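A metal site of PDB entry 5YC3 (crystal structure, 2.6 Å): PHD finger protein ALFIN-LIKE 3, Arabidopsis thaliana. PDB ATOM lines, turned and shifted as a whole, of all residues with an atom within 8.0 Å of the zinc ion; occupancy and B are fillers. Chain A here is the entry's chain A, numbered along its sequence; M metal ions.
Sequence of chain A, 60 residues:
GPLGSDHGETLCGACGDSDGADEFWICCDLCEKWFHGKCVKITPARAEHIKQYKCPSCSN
The zinc ion is bound by SG of Cys 55 (2.3 Å), SG of Cys 58 (2.4 Å), SG of Cys 31 (2.4 Å) and SG of Cys 28 (2.4 Å).
The backbone NH of Lys 33 lies close to the side-chain sulfur of Cys 31, 3.6 Å away. The side-chain sulfur of Cys 55 lies close to the backbone NH of Ser 57, at 3.7 Å. O of Lys 33 lies within hydrogen-bond range of N of Cys 28, at 3.0 Å. The side-chain sulfur (SG) of Cys 28 sits close to the backbone NH (N) of Leu 30 (3.4 Å). O of Cys 55 sits at hydrogen-bond distance from OG of Ser 59, at 2.9 Å.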
ATOM      1  N   CYS A  27     -10.855  15.079 -15.991  1.00  0.00           N
ATOM      2  CA  CYS A  27     -12.251  14.897 -15.629  1.00  0.00           C
ATOM      3  C   CYS A  27     -13.092  14.415 -16.809  1.00  0.00           C
ATOM      4  O   CYS A  27     -12.963  14.920 -17.924  1.00  0.00           O
ATOM      5  CB  CYS A  27     -12.829  16.196 -15.080  1.00  0.00           C
ATOM      6  SG  CYS A  27     -14.397  16.027 -14.222  1.00  0.00           S
ATOM      7  N   CYS A  28     -13.963  13.449 -16.551  1.00  0.00           N
ATOM      8  CA  CYS A  28     -14.896  12.965 -17.573  1.00  0.00           C
ATOM      9  C   CYS A  28     -16.037  13.962 -17.763  1.00  0.00           C
ATOM     10  O   CYS A  28     -16.646  14.394 -16.793  1.00  0.00           O
ATOM     11  CB  CYS A  28     -15.443  11.596 -17.177  1.00  0.00           C
ATOM     12  SG  CYS A  28     -16.684  10.941 -18.306  1.00  0.00           S
ATOM     13  N   ASP A  29     -16.314  14.340 -19.005  1.00  0.00           N
ATOM     14  CA  ASP A  29     -17.327  15.352 -19.256  1.00  0.00           C
ATOM     15  C   ASP A  29     -18.762  14.807 -19.173  1.00  0.00           C
ATOM     16  O   ASP A  29     -19.721  15.569 -19.250  1.00  0.00           O
ATOM     17  CB  ASP A  29     -17.101  16.008 -20.622  1.00  0.00           C
ATOM     18  CG  ASP A  29     -15.998  17.054 -20.593  1.00  0.00           C
ATOM     19  OD1 ASP A  29     -15.635  17.511 -19.489  1.00  0.00           O
ATOM     20  OD2 ASP A  29     -15.504  17.431 -21.683  1.00  0.00           O
ATOM     21  N   LEU A  30     -18.889  13.491 -19.015  1.00  0.00           N
ATOM     22  CA  LEU A  30     -20.211  12.881 -18.990  1.00  0.00           C
ATOM     23  C   LEU A  30     -20.694  12.551 -17.574  1.00  0.00           C
ATOM     24  O   LEU A  30     -21.840  12.848 -17.237  1.00  0.00           O
ATOM     25  CB  LEU A  30     -20.232  11.619 -19.859  1.00  0.00           C
ATOM     26  CG  LEU A  30     -20.183  11.856 -21.375  1.00  0.00           C
ATOM     27  CD1 LEU A  30     -20.636  10.617 -22.118  1.00  0.00           C
ATOM     28  CD2 LEU A  30     -21.031  13.059 -21.777  1.00  0.00           C
ATOM     29  N   CYS A  31     -19.833  11.955 -16.765  1.00  0.00           N
ATOM     30  CA  CYS A  31     -20.211  11.591 -15.401  1.00  0.00           C
ATOM     31  C   CYS A  31     -19.560  12.526 -14.385  1.00  0.00           C
ATOM     32  O   CYS A  31     -19.876  12.497 -13.195  1.00  0.00           O
ATOM     33  CB  CYS A  31     -19.835  10.137 -15.094  1.00  0.00           C
ATOM     34  SG  CYS A  31     -18.065   9.831 -14.853  1.00  0.00           S
ATOM     35  N   GLU A  32     -18.631  13.353 -14.870  1.00  0.00           N
ATOM     36  CA  GLU A  32     -17.928  14.355 -14.060  1.00  0.00           C
ATOM     37  C   GLU A  32     -17.108  13.761 -12.914  1.00  0.00           C
ATOM     38  O   GLU A  32     -16.958  14.383 -11.870  1.00  0.00           O
ATOM     39  CB  GLU A  32     -18.915  15.381 -13.525  1.00  0.00           C
ATOM     40  CG  GLU A  32     -19.525  16.235 -14.621  1.00  0.00           C
ATOM     41  CD  GLU A  32     -20.448  17.319 -14.078  1.00  0.00           C
ATOM     42  OE1 GLU A  32     -21.335  16.995 -13.254  1.00  0.00           O
ATOM     43  OE2 GLU A  32     -20.274  18.495 -14.483  1.00  0.00           O
ATOM     44  N   LYS A  33     -16.555  12.573 -13.133  1.00  0.00           N
ATOM     45  CA  LYS A  33     -15.596  11.990 -12.201  1.00  0.00           C
ATOM     46  C   LYS A  33     -14.180  12.458 -12.535  1.00  0.00           C
ATOM     47  O   LYS A  33     -13.849  12.692 -13.694  1.00  0.00           O
ATOM     48  CB  LYS A  33     -15.666  10.462 -12.218  1.00  0.00           C
ATOM     49  CG  LYS A  33     -16.889   9.874 -11.525  1.00  0.00           C
ATOM     50  CD  LYS A  33     -16.861   8.351 -11.610  1.00  0.00           C
ATOM     51  CE  LYS A  33     -18.111   7.734 -10.992  1.00  0.00           C
ATOM     52  NZ  LYS A  33     -18.116   6.242 -11.151  1.00  0.00           N
ATOM     53  N   TRP A  34     -13.340  12.584 -11.505  1.00  0.00           N
ATOM     54  CA  TRP A  34     -11.943  12.942 -11.700  1.00  0.00           C
ATOM     55  C   TRP A  34     -11.066  11.706 -11.650  1.00  0.00           C
ATOM     56  O   TRP A  34     -11.382  10.731 -10.972  1.00  0.00           O
ATOM     57  CB  TRP A  34     -11.486  13.945 -10.640  1.00  0.00           C
ATOM     58  CG  TRP A  34     -11.843  15.369 -10.934  1.00  0.00           C
ATOM     59  CD1 TRP A  34     -12.903  16.079 -10.440  1.00  0.00           C
ATOM     60  CD2 TRP A  34     -11.110  16.265 -11.781  1.00  0.00           C
ATOM     61  NE1 TRP A  34     -12.878  17.362 -10.931  1.00  0.00           N
ATOM     62  CE2 TRP A  34     -11.792  17.503 -11.753  1.00  0.00           C
ATOM     63  CE3 TRP A  34      -9.957  16.147 -12.549  1.00  0.00           C
ATOM     64  CZ2 TRP A  34     -11.360  18.606 -12.478  1.00  0.00           C
ATOM     65  CZ3 TRP A  34      -9.526  17.251 -13.274  1.00  0.00           C
ATOM     66  CH2 TRP A  34     -10.218  18.460 -13.231  1.00  0.00           C
ATOM     67  N   PHE A  35      -9.950  11.759 -12.370  1.00  0.00           N
ATOM     68  CA  PHE A  35      -9.023  10.633 -12.441  1.00  0.00           C
ATOM     69  C   PHE A  35      -7.577  11.092 -12.421  1.00  0.00           C
ATOM     70  O   PHE A  35      -7.222  12.064 -13.102  1.00  0.00           O
ATOM     71  CB  PHE A  35      -9.269   9.802 -13.701  1.00  0.00           C
ATOM     72  CG  PHE A  35     -10.648   9.197 -13.796  1.00  0.00           C
ATOM     73  CD1 PHE A  35     -11.697   9.913 -14.346  1.00  0.00           C
ATOM     74  CD2 PHE A  35     -10.886   7.911 -13.341  1.00  0.00           C
ATOM     75  CE1 PHE A  35     -12.973   9.354 -14.434  1.00  0.00           C
ATOM     76  CE2 PHE A  35     -12.142   7.351 -13.429  1.00  0.00           C
ATOM     77  CZ  PHE A  35     -13.190   8.068 -13.970  1.00  0.00           C
ATOM     78  N   TYR A  53     -13.023  14.625 -22.525  1.00  0.00           N
ATOM     79  CA  TYR A  53     -12.637  13.312 -22.016  1.00  0.00           C
ATOM     80  C   TYR A  53     -13.848  12.505 -21.566  1.00  0.00           C
ATOM     81  O   TYR A  53     -14.729  13.005 -20.851  1.00  0.00           O
ATOM     82  CB  TYR A  53     -11.650  13.430 -20.853  1.00  0.00           C
ATOM     83  CG  TYR A  53     -11.256  12.078 -20.329  1.00  0.00           C
ATOM     84  CD1 TYR A  53     -10.662  11.141 -21.164  1.00  0.00           C
ATOM     85  CD2 TYR A  53     -11.485  11.720 -19.007  1.00  0.00           C
ATOM     86  CE1 TYR A  53     -10.304   9.893 -20.704  1.00  0.00           C
ATOM     87  CE2 TYR A  53     -11.127  10.464 -18.534  1.00  0.00           C
ATOM     88  CZ  TYR A  53     -10.542   9.556 -19.383  1.00  0.00           C
ATOM     89  OH  TYR A  53     -10.176   8.305 -18.943  1.00  0.00           O
ATOM     90  N   LYS A  54     -13.873  11.249 -21.990  1.00  0.00           N
ATOM     91  CA  LYS A  54     -14.926  10.320 -21.623  1.00  0.00           C
ATOM     92  C   LYS A  54     -14.298   9.082 -20.990  1.00  0.00           C
ATOM     93  O   LYS A  54     -13.538   8.357 -21.634  1.00  0.00           O
ATOM     94  CB  LYS A  54     -15.753   9.951 -22.852  1.00  0.00           C
ATOM     95  CG  LYS A  54     -16.950   9.063 -22.603  1.00  0.00           C
ATOM     96  CD  LYS A  54     -17.871   9.085 -23.821  1.00  0.00           C
ATOM     97  CE  LYS A  54     -17.076   8.851 -25.096  1.00  0.00           C
ATOM     98  NZ  LYS A  54     -17.943   8.780 -26.314  1.00  0.00           N
ATOM     99  N   CYS A  55     -14.590   8.863 -19.713  1.00  0.00           N
ATOM    100  CA  CYS A  55     -13.950   7.822 -18.916  1.00  0.00           C
ATOM    101  C   CYS A  55     -14.301   6.434 -19.462  1.00  0.00           C
ATOM    102  O   CYS A  55     -15.267   6.303 -20.229  1.00  0.00           O
ATOM    103  CB  CYS A  55     -14.358   7.962 -17.441  1.00  0.00           C
ATOM    104  SG  CYS A  55     -16.020   7.393 -17.066  1.00  0.00           S
ATOM    105  N   PRO A  56     -13.524   5.401 -19.100  1.00  0.00           N
ATOM    106  CA  PRO A  56     -13.769   4.031 -19.554  1.00  0.00           C
ATOM    107  C   PRO A  56     -15.203   3.548 -19.328  1.00  0.00           C
ATOM    108  O   PRO A  56     -15.795   2.933 -20.213  1.00  0.00           O
ATOM    109  CB  PRO A  56     -12.800   3.203 -18.699  1.00  0.00           C
ATOM    110  CG  PRO A  56     -11.680   4.134 -18.412  1.00  0.00           C
ATOM    111  CD  PRO A  56     -12.288   5.492 -18.294  1.00  0.00           C
ATOM    112  N   SER A  57     -15.760   3.834 -18.158  1.00  0.00           N
ATOM    113  CA  SER A  57     -17.114   3.401 -17.833  1.00  0.00           C
ATOM    114  C   SER A  57     -18.149   4.042 -18.749  1.00  0.00           C
ATOM    115  O   SER A  57     -19.081   3.370 -19.197  1.00  0.00           O
ATOM    116  CB  SER A  57     -17.431   3.737 -16.373  1.00  0.00           C
ATOM    117  OG  SER A  57     -18.763   3.351 -16.066  1.00  0.00           O
ATOM    118  N   CYS A  58     -17.991   5.329 -19.026  1.00  0.00           N
ATOM    119  CA  CYS A  58     -18.946   6.047 -19.867  1.00  0.00           C
ATOM    120  C   CYS A  58     -18.792   5.689 -21.334  1.00  0.00           C
ATOM    121  O   CYS A  58     -19.721   5.837 -22.124  1.00  0.00           O
ATOM    122  CB  CYS A  58     -18.787   7.566 -19.672  1.00  0.00           C
ATOM    123  SG  CYS A  58     -19.441   8.179 -18.108  1.00  0.00           S
ATOM    124  N   SER A  59     -17.621   5.185 -21.693  1.00  0.00           N
ATOM    125  CA  SER A  59     -17.341   4.822 -23.077  1.00  0.00           C
ATOM    126  C   SER A  59     -17.923   3.462 -23.459  1.00  0.00           C
ATOM    127  O   SER A  59     -17.616   2.932 -24.527  1.00  0.00           O
ATOM    128  CB  SER A  59     -15.830   4.831 -23.331  1.00  0.00           C
ATOM    129  OG  SER A  59     -15.283   6.117 -23.128  1.00  0.00           O
HETATM  130 ZN    ZN M   1     -17.526   9.079 -17.049  1.00  0.00          ZN
